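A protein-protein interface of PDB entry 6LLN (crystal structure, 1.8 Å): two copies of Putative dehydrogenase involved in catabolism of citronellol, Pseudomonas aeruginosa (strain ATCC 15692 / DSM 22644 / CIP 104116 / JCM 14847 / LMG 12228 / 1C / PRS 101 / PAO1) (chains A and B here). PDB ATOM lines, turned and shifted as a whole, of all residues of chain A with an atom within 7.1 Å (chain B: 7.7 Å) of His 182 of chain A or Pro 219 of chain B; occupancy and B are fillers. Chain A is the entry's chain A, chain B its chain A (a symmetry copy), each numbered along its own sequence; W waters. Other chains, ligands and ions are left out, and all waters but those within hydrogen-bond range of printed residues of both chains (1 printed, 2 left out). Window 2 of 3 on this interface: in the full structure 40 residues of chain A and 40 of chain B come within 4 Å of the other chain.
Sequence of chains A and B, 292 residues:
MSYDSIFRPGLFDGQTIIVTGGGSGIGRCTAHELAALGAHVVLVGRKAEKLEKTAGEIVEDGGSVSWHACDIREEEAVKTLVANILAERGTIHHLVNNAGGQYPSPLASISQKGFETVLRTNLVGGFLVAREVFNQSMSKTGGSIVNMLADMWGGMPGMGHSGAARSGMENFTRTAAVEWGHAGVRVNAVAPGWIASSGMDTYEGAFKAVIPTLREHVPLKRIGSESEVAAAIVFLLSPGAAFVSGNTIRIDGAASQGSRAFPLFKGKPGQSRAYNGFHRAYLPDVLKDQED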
ATOM      1  N   PHE A 134       6.839 -33.846 -16.649  1.00  0.00           N
ATOM      2  CA  PHE A 134       6.235 -33.940 -15.324  1.00  0.00           C
ATOM      3  C   PHE A 134       6.288 -35.378 -14.802  1.00  0.00           C
ATOM      4  O   PHE A 134       6.797 -35.635 -13.705  1.00  0.00           O
ATOM      5  CB  PHE A 134       4.791 -33.434 -15.370  1.00  0.00           C
ATOM      6  CG  PHE A 134       4.101 -33.437 -14.035  1.00  0.00           C
ATOM      7  CD1 PHE A 134       4.449 -32.518 -13.058  1.00  0.00           C
ATOM      8  CD2 PHE A 134       3.106 -34.365 -13.751  1.00  0.00           C
ATOM      9  CE1 PHE A 134       3.813 -32.511 -11.823  1.00  0.00           C
ATOM     10  CE2 PHE A 134       2.460 -34.359 -12.520  1.00  0.00           C
ATOM     11  CZ  PHE A 134       2.818 -33.436 -11.553  1.00  0.00           C
ATOM     12  N   SER A 139       7.420 -34.014 -11.464  1.00  0.00           N
ATOM     13  CA  SER A 139       6.485 -34.321 -10.383  1.00  0.00           C
ATOM     14  C   SER A 139       7.200 -34.646  -9.075  1.00  0.00           C
ATOM     15  O   SER A 139       6.580 -34.579  -8.009  1.00  0.00           O
ATOM     16  CB  SER A 139       5.566 -35.490 -10.770  1.00  0.00           C
ATOM     17  OG  SER A 139       6.315 -36.678 -11.007  1.00  0.00           O
ATOM     18  N   ARG A 174      -3.099 -23.166 -17.808  1.00  0.00           N
ATOM     19  CA  ARG A 174      -3.816 -22.911 -16.557  1.00  0.00           C
ATOM     20  C   ARG A 174      -4.145 -24.216 -15.837  1.00  0.00           C
ATOM     21  O   ARG A 174      -3.973 -24.327 -14.617  1.00  0.00           O
ATOM     22  CB  ARG A 174      -5.108 -22.138 -16.840  1.00  0.00           C
ATOM     23  CG  ARG A 174      -4.961 -20.731 -17.453  1.00  0.00           C
ATOM     24  CD  ARG A 174      -6.375 -20.277 -17.886  1.00  0.00           C
ATOM     25  NE  ARG A 174      -6.405 -19.197 -18.856  1.00  0.00           N
ATOM     26  CZ  ARG A 174      -7.006 -18.022 -18.659  1.00  0.00           C
ATOM     27  NH1 ARG A 174      -7.615 -17.755 -17.507  1.00  0.00           N
ATOM     28  NH2 ARG A 174      -6.980 -17.103 -19.614  1.00  0.00           N
ATOM     29  N   ALA A 176      -2.697 -27.147 -16.036  1.00  0.00           N
ATOM     30  CA  ALA A 176      -1.484 -27.751 -15.492  1.00  0.00           C
ATOM     31  C   ALA A 176      -0.943 -26.952 -14.311  1.00  0.00           C
ATOM     32  O   ALA A 176      -0.440 -27.531 -13.338  1.00  0.00           O
ATOM     33  CB  ALA A 176      -0.432 -27.874 -16.594  1.00  0.00           C
ATOM     34  N   ALA A 177      -1.042 -25.616 -14.357  1.00  0.00           N
ATOM     35  CA  ALA A 177      -0.628 -24.839 -13.191  1.00  0.00           C
ATOM     36  C   ALA A 177      -1.422 -25.250 -11.953  1.00  0.00           C
ATOM     37  O   ALA A 177      -0.865 -25.365 -10.853  1.00  0.00           O
ATOM     38  CB  ALA A 177      -0.790 -23.342 -13.467  1.00  0.00           C
ATOM     39  N   VAL A 178      -2.722 -25.491 -12.122  1.00  0.00           N
ATOM     40  CA  VAL A 178      -3.550 -25.904 -10.997  1.00  0.00           C
ATOM     41  C   VAL A 178      -3.216 -27.337 -10.589  1.00  0.00           C
ATOM     42  O   VAL A 178      -2.950 -27.615  -9.416  1.00  0.00           O
ATOM     43  CB  VAL A 178      -5.042 -25.742 -11.335  1.00  0.00           C
ATOM     44  CG1 VAL A 178      -5.901 -26.243 -10.172  1.00  0.00           C
ATOM     45  CG2 VAL A 178      -5.364 -24.273 -11.631  1.00  0.00           C
ATOM     46  N   GLU A 179      -3.192 -28.261 -11.553  1.00  0.00           N
ATOM     47  CA  GLU A 179      -3.043 -29.678 -11.212  1.00  0.00           C
ATOM     48  C   GLU A 179      -1.642 -30.019 -10.705  1.00  0.00           C
ATOM     49  O   GLU A 179      -1.492 -30.949  -9.908  1.00  0.00           O
ATOM     50  CB  GLU A 179      -3.376 -30.554 -12.419  1.00  0.00           C
ATOM     51  CG  GLU A 179      -4.837 -30.537 -12.815  1.00  0.00           C
ATOM     52  CD  GLU A 179      -5.202 -31.679 -13.759  1.00  0.00           C
ATOM     53  OE1 GLU A 179      -4.421 -32.653 -13.865  1.00  0.00           O
ATOM     54  OE2 GLU A 179      -6.270 -31.596 -14.395  1.00  0.00           O
ATOM     55  N   TRP A 180      -0.607 -29.303 -11.149  1.00  0.00           N
ATOM     56  CA  TRP A 180       0.767 -29.678 -10.835  1.00  0.00           C
ATOM     57  C   TRP A 180       1.412 -28.782  -9.793  1.00  0.00           C
ATOM     58  O   TRP A 180       2.543 -29.063  -9.376  1.00  0.00           O
ATOM     59  CB  TRP A 180       1.612 -29.698 -12.117  1.00  0.00           C
ATOM     60  CG  TRP A 180       1.115 -30.694 -13.121  1.00  0.00           C
ATOM     61  CD1 TRP A 180       0.158 -31.655 -12.920  1.00  0.00           C
ATOM     62  CD2 TRP A 180       1.532 -30.827 -14.485  1.00  0.00           C
ATOM     63  NE1 TRP A 180      -0.037 -32.377 -14.075  1.00  0.00           N
ATOM     64  CE2 TRP A 180       0.803 -31.894 -15.045  1.00  0.00           C
ATOM     65  CE3 TRP A 180       2.466 -30.158 -15.282  1.00  0.00           C
ATOM     66  CZ2 TRP A 180       0.963 -32.291 -16.371  1.00  0.00           C
ATOM     67  CZ3 TRP A 180       2.623 -30.555 -16.599  1.00  0.00           C
ATOM     68  CH2 TRP A 180       1.885 -31.615 -17.129  1.00  0.00           C
ATOM     69  N   GLY A 181       0.720 -27.721  -9.361  1.00  0.00           N
ATOM     70  CA  GLY A 181       1.271 -26.817  -8.362  1.00  0.00           C
ATOM     71  C   GLY A 181       1.678 -27.508  -7.075  1.00  0.00           C
ATOM     72  O   GLY A 181       2.645 -27.100  -6.428  1.00  0.00           O
ATOM     73  N   HIS A 182       0.948 -28.554  -6.679  1.00  0.00           N
ATOM     74  CA  HIS A 182       1.290 -29.262  -5.447  1.00  0.00           C
ATOM     75  C   HIS A 182       2.685 -29.867  -5.522  1.00  0.00           C
ATOM     76  O   HIS A 182       3.352 -30.012  -4.494  1.00  0.00           O
ATOM     77  CB  HIS A 182       0.254 -30.351  -5.159  1.00  0.00           C
ATOM     78  CG  HIS A 182       0.378 -31.542  -6.058  1.00  0.00           C
ATOM     79  ND1 HIS A 182      -0.242 -31.615  -7.288  1.00  0.00           N
ATOM     80  CD2 HIS A 182       1.062 -32.702  -5.913  1.00  0.00           C
ATOM     81  CE1 HIS A 182       0.055 -32.768  -7.862  1.00  0.00           C
ATOM     82  NE2 HIS A 182       0.846 -33.445  -7.047  1.00  0.00           N
ATOM     83  N   ALA A 183       3.162 -30.188  -6.724  1.00  0.00           N
ATOM     84  CA  ALA A 183       4.501 -30.739  -6.875  1.00  0.00           C
ATOM     85  C   ALA A 183       5.582 -29.668  -6.990  1.00  0.00           C
ATOM     86  O   ALA A 183       6.734 -30.005  -7.267  1.00  0.00           O
ATOM     87  CB  ALA A 183       4.556 -31.663  -8.094  1.00  0.00           C
ATOM     88  N   GLY A 184       5.249 -28.396  -6.774  1.00  0.00           N
ATOM     89  CA  GLY A 184       6.239 -27.348  -6.949  1.00  0.00           C
ATOM     90  C   GLY A 184       6.513 -27.021  -8.397  1.00  0.00           C
ATOM     91  O   GLY A 184       7.603 -26.545  -8.731  1.00  0.00           O
ATOM     92  N   VAL A 185       5.552 -27.272  -9.277  1.00  0.00           N
ATOM     93  CA  VAL A 185       5.723 -27.070 -10.708  1.00  0.00           C
ATOM     94  C   VAL A 185       4.900 -25.848 -11.102  1.00  0.00           C
ATOM     95  O   VAL A 185       3.688 -25.805 -10.871  1.00  0.00           O
ATOM     96  CB  VAL A 185       5.311 -28.312 -11.508  1.00  0.00           C
ATOM     97  CG1 VAL A 185       5.447 -28.053 -12.995  1.00  0.00           C
ATOM     98  CG2 VAL A 185       6.204 -29.515 -11.123  1.00  0.00           C
ATOM     99  N   SER A 245       2.428 -18.457 -11.672  1.00  0.00           N
ATOM    100  CA  SER A 245       1.994 -19.708 -12.288  1.00  0.00           C
ATOM    101  C   SER A 245       0.596 -19.523 -12.868  1.00  0.00           C
ATOM    102  O   SER A 245      -0.244 -18.838 -12.278  1.00  0.00           O
ATOM    103  CB  SER A 245       2.008 -20.867 -11.285  1.00  0.00           C
ATOM    104  OG  SER A 245       1.929 -22.117 -11.967  1.00  0.00           O
ATOM    105  N   TRP B 194      -2.166 -13.533  -2.806  1.00  0.00           N
ATOM    106  CA  TRP B 194      -1.945 -13.494  -1.366  1.00  0.00           C
ATOM    107  C   TRP B 194      -0.445 -13.391  -1.112  1.00  0.00           C
ATOM    108  O   TRP B 194       0.303 -14.346  -1.352  1.00  0.00           O
ATOM    109  CB  TRP B 194      -2.561 -14.723  -0.703  1.00  0.00           C
ATOM    110  CG  TRP B 194      -4.067 -14.705  -0.809  1.00  0.00           C
ATOM    111  CD1 TRP B 194      -4.904 -13.727  -0.351  1.00  0.00           C
ATOM    112  CD2 TRP B 194      -4.905 -15.683  -1.440  1.00  0.00           C
ATOM    113  NE1 TRP B 194      -6.209 -14.041  -0.643  1.00  0.00           N
ATOM    114  CE2 TRP B 194      -6.236 -15.235  -1.315  1.00  0.00           C
ATOM    115  CE3 TRP B 194      -4.660 -16.894  -2.095  1.00  0.00           C
ATOM    116  CZ2 TRP B 194      -7.321 -15.959  -1.816  1.00  0.00           C
ATOM    117  CZ3 TRP B 194      -5.741 -17.611  -2.594  1.00  0.00           C
ATOM    118  CH2 TRP B 194      -7.052 -17.139  -2.451  1.00  0.00           C
ATOM    119  N   GLU B 216      -4.495 -22.207   1.672  1.00  0.00           N
ATOM    120  CA  GLU B 216      -4.164 -23.477   1.035  1.00  0.00           C
ATOM    121  C   GLU B 216      -5.116 -23.746  -0.131  1.00  0.00           C
ATOM    122  O   GLU B 216      -5.204 -24.879  -0.621  1.00  0.00           O
ATOM    123  CB  GLU B 216      -4.181 -24.640   2.040  1.00  0.00           C
ATOM    124  CG  GLU B 216      -3.581 -25.938   1.496  1.00  0.00           C
ATOM    125  CD  GLU B 216      -3.938 -27.162   2.305  1.00  0.00           C
ATOM    126  OE1 GLU B 216      -5.103 -27.609   2.228  1.00  0.00           O
ATOM    127  OE2 GLU B 216      -3.040 -27.705   2.984  1.00  0.00           O
ATOM    128  N   HIS B 217      -5.845 -22.731  -0.580  1.00  0.00           N
ATOM    129  CA  HIS B 217      -6.464 -22.754  -1.896  1.00  0.00           C
ATOM    130  C   HIS B 217      -5.571 -22.099  -2.944  1.00  0.00           C
ATOM    131  O   HIS B 217      -6.062 -21.490  -3.907  1.00  0.00           O
ATOM    132  CB  HIS B 217      -7.845 -22.110  -1.816  1.00  0.00           C
ATOM    133  CG  HIS B 217      -8.690 -22.685  -0.720  1.00  0.00           C
ATOM    134  ND1 HIS B 217      -8.579 -23.999  -0.321  1.00  0.00           N
ATOM    135  CD2 HIS B 217      -9.625 -22.125   0.085  1.00  0.00           C
ATOM    136  CE1 HIS B 217      -9.420 -24.231   0.670  1.00  0.00           C
ATOM    137  NE2 HIS B 217     -10.067 -23.111   0.936  1.00  0.00           N
ATOM    138  N   VAL B 218      -4.266 -22.199  -2.744  1.00  0.00           N
ATOM    139  CA  VAL B 218      -3.223 -21.814  -3.694  1.00  0.00           C
ATOM    140  C   VAL B 218      -2.630 -23.098  -4.245  1.00  0.00           C
ATOM    141  O   VAL B 218      -2.158 -23.936  -3.463  1.00  0.00           O
ATOM    142  CB  VAL B 218      -2.133 -20.958  -3.025  1.00  0.00           C
ATOM    143  CG1 VAL B 218      -1.102 -20.524  -4.053  1.00  0.00           C
ATOM    144  CG2 VAL B 218      -2.735 -19.759  -2.305  1.00  0.00           C
ATOM    145  N   PRO B 219      -2.628 -23.313  -5.564  1.00  0.00           N
ATOM    146  CA  PRO B 219      -2.040 -24.555  -6.097  1.00  0.00           C
ATOM    147  C   PRO B 219      -0.601 -24.789  -5.664  1.00  0.00           C
ATOM    148  O   PRO B 219      -0.223 -25.940  -5.410  1.00  0.00           O
ATOM    149  CB  PRO B 219      -2.176 -24.365  -7.613  1.00  0.00           C
ATOM    150  CG  PRO B 219      -3.423 -23.563  -7.744  1.00  0.00           C
ATOM    151  CD  PRO B 219      -3.376 -22.574  -6.597  1.00  0.00           C
ATOM    152  N   LEU B 220       0.216 -23.733  -5.568  1.00  0.00           N
ATOM    153  CA  LEU B 220       1.579 -23.890  -5.070  1.00  0.00           C
ATOM    154  C   LEU B 220       1.628 -24.086  -3.559  1.00  0.00           C
ATOM    155  O   LEU B 220       2.712 -24.334  -3.023  1.00  0.00           O
ATOM    156  CB  LEU B 220       2.437 -22.679  -5.457  1.00  0.00           C
ATOM    157  CG  LEU B 220       2.880 -22.516  -6.921  1.00  0.00           C
ATOM    158  CD1 LEU B 220       3.747 -21.272  -7.068  1.00  0.00           C
ATOM    159  CD2 LEU B 220       3.642 -23.728  -7.408  1.00  0.00           C
ATOM    160  N   LYS B 221       0.492 -23.964  -2.871  1.00  0.00           N
ATOM    161  CA  LYS B 221       0.354 -24.326  -1.460  1.00  0.00           C
ATOM    162  C   LYS B 221       1.207 -23.457  -0.543  1.00  0.00           C
ATOM    163  O   LYS B 221       1.699 -23.926   0.483  1.00  0.00           O
ATOM    164  CB  LYS B 221       0.680 -25.806  -1.232  1.00  0.00           C
ATOM    165  CG  LYS B 221      -0.253 -26.763  -1.966  1.00  0.00           C
ATOM    166  CD  LYS B 221      -1.616 -26.842  -1.295  1.00  0.00           C
ATOM    167  CE  LYS B 221      -2.352 -28.131  -1.661  1.00  0.00           C
ATOM    168  NZ  LYS B 221      -3.486 -28.414  -0.730  1.00  0.00           N
ATOM    169  N   ARG B 222       1.390 -22.189  -0.895  1.00  0.00           N
ATOM    170  CA  ARG B 222       2.074 -21.260  -0.012  1.00  0.00           C
ATOM    171  C   ARG B 222       1.636 -19.848  -0.364  1.00  0.00           C
ATOM    172  O   ARG B 222       0.976 -19.610  -1.379  1.00  0.00           O
ATOM    173  CB  ARG B 222       3.593 -21.401  -0.112  1.00  0.00           C
ATOM    174  CG  ARG B 222       4.151 -21.096  -1.483  1.00  0.00           C
ATOM    175  CD  ARG B 222       5.663 -21.022  -1.442  1.00  0.00           C
ATOM    176  NE  ARG B 222       6.257 -20.707  -2.740  1.00  0.00           N
ATOM    177  CZ  ARG B 222       6.494 -19.472  -3.169  1.00  0.00           C
ATOM    178  NH1 ARG B 222       6.177 -18.429  -2.408  1.00  0.00           N
ATOM    179  NH2 ARG B 222       7.055 -19.272  -4.352  1.00  0.00           N
ATOM    180  N   ASP B 252       0.195 -14.916  -8.202  1.00  0.00           N
ATOM    181  CA  ASP B 252      -0.792 -15.430  -7.257  1.00  0.00           C
ATOM    182  C   ASP B 252      -0.674 -16.939  -7.056  1.00  0.00           C
ATOM    183  O   ASP B 252      -1.616 -17.558  -6.557  1.00  0.00           O
ATOM    184  CB  ASP B 252      -2.232 -15.075  -7.697  1.00  0.00           C
ATOM    185  CG  ASP B 252      -2.567 -15.566  -9.111  1.00  0.00           C
ATOM    186  OD1 ASP B 252      -1.931 -16.528  -9.576  1.00  0.00           O
ATOM    187  OD2 ASP B 252      -3.467 -14.982  -9.773  1.00  0.00           O
ATOM    188  N   GLY B 253       0.439 -17.548  -7.463  1.00  0.00           N
ATOM    189  CA  GLY B 253       0.614 -18.982  -7.298  1.00  0.00           C
ATOM    190  C   GLY B 253      -0.405 -19.835  -8.022  1.00  0.00           C
ATOM    191  O   GLY B 253      -0.589 -21.001  -7.656  1.00  0.00           O
ATOM    192  N   ALA B 254      -1.050 -19.283  -9.060  1.00  0.00           N
ATOM    193  CA  ALA B 254      -2.154 -19.870  -9.831  1.00  0.00           C
ATOM    194  C   ALA B 254      -3.472 -19.894  -9.058  1.00  0.00           C
ATOM    195  O   ALA B 254      -4.417 -20.576  -9.467  1.00  0.00           O
ATOM    196  CB  ALA B 254      -1.824 -21.276 -10.350  1.00  0.00           C
ATOM    197  N   ALA B 255      -3.578 -19.109  -7.986  1.00  0.00           N
ATOM    198  CA  ALA B 255      -4.805 -19.103  -7.192  1.00  0.00           C
ATOM    199  C   ALA B 255      -5.993 -18.566  -7.978  1.00  0.00           C
ATOM    200  O   ALA B 255      -7.142 -18.924  -7.682  1.00  0.00           O
ATOM    201  CB  ALA B 255      -4.597 -18.291  -5.916  1.00  0.00           C
ATOM    202  N   SER B 256      -5.752 -17.714  -8.975  1.00  0.00           N
ATOM    203  CA  SER B 256      -6.858 -17.217  -9.785  1.00  0.00           C
ATOM    204  C   SER B 256      -7.345 -18.231 -10.812  1.00  0.00           C
ATOM    205  O   SER B 256      -8.371 -17.986 -11.453  1.00  0.00           O
ATOM    206  CB  SER B 256      -6.466 -15.921 -10.498  1.00  0.00           C
ATOM    207  OG  SER B 256      -5.293 -16.099 -11.279  1.00  0.00           O
ATOM    208  N   GLN B 257      -6.658 -19.358 -10.984  1.00  0.00           N
ATOM    209  CA  GLN B 257      -7.097 -20.324 -11.993  1.00  0.00           C
ATOM    210  C   GLN B 257      -7.941 -21.430 -11.358  1.00  0.00           C
ATOM    211  O   GLN B 257      -7.999 -21.538 -10.133  1.00  0.00           O
ATOM    212  CB  GLN B 257      -5.905 -20.933 -12.736  1.00  0.00           C
ATOM    213  CG  GLN B 257      -4.894 -19.928 -13.267  1.00  0.00           C
ATOM    214  CD  GLN B 257      -5.465 -18.953 -14.285  1.00  0.00           C
ATOM    215  OE1 GLN B 257      -4.908 -17.869 -14.497  1.00  0.00           O
ATOM    216  NE2 GLN B 257      -6.556 -19.331 -14.927  1.00  0.00           N
HETATM  217  O   HOH W   1       0.625 -16.116 -10.937  1.00  0.00           O
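Among the printed residues, pairs that only touch across the chains: Ala 177 of chain A with Pro 219 of chain B (3.6 Å), Ala 177 of chain A with Ala 254 of chain B (3.9 Å), Val 178 of chain A with Pro 219 of chain B (3.8 Å), Val 178 of chain A with Gln 257 of chain B (3.6 Å), Gly 181 of chain A with Leu 220 of chain B (3.6 Å) and Ser 245 of chain A with Asp 252 of chain B (3.9 Å).
Printed residues of chain B within 4 Å of Arg 174 of chain A: Gln 257 (3.1 Å). Of the printed residues of chain B, Ala 177 of chain A touches Pro 219 and Ala 254. Gly 181 of chain A touches just these residues of chain B: Pro 219 and Leu 220. Of chain B, only Pro 219 comes within 4 Å of His 182 of chain A. Of the printed residues of chain B, Ser 245 of chain A touches Asp 252 (3.9 Å) and Ala 254 (3.3 Å). Pro 219 of chain B touches four residues of chain A. Printed residues of chain A within 4 Å of Leu 220 of chain B: Gly 181. Arg 222 of chain B touches none of the printed residues of chain A. Ala 255 of chain B touches none of the printed residues of chain A. The nearest residue of chain B that does not touch His 182 of chain A is Lys 221 of chain B (4.6 Å). The nearest residue of chain A that does not touch Pro 219 of chain B is Trp 180 of chain A (5.5 Å). The nearest printed residue of chain B that does not touch Arg 174 of chain A is Ala 254 of chain B (5.7 Å).
OD1 of Asp 252 of chain B sits at hydrogen-bond distance from N of Ala 255 of chain B (3.4 Å). The backbone carbonyl oxygen (O) of Glu 179 of chain A lies within hydrogen-bond range of a ring nitrogen (ND1) of His 182 of chain A, 3.0 Å away. OD2 of Asp 252 of chain B sits at hydrogen-bond distance from OG of Ser 256 of chain B (2.6 Å). OD1 of Asp 252 of chain B is in hydrogen-bond range of N of Ala 254 of chain B (2.9 Å).
The backbone NH (N) of His 182 of chain A lies within hydrogen-bond range of the backbone carbonyl oxygen (O) of Pro 219 of chain B (3.1 Å). NE2 of Gln 257 of chain B sits close to NH1 of Arg 174 of chain A (3.2 Å). O of Ser 245 of chain A sits close to N of Ala 254 of chain B, at 3.3 Å. The backbone carbonyl oxygen (O) of Gly 181 of chain A lies close to the backbone carbonyl oxygen (O) of Pro 219 of chain B (3.3 Å).
No position is printed for both chains.
Water W1 lies within hydrogen-bond range of OD1 of Asp 252 of chain B (2.9 Å) and N of Ser 245 of chain A (3.0 Å).
Of the 14 printed residues of chain A, 6 touch a printed residue of chain B. Hydrophobic or aromatic side chains of chain A that line the printed part of chain B: Ala 177 and Val 178.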
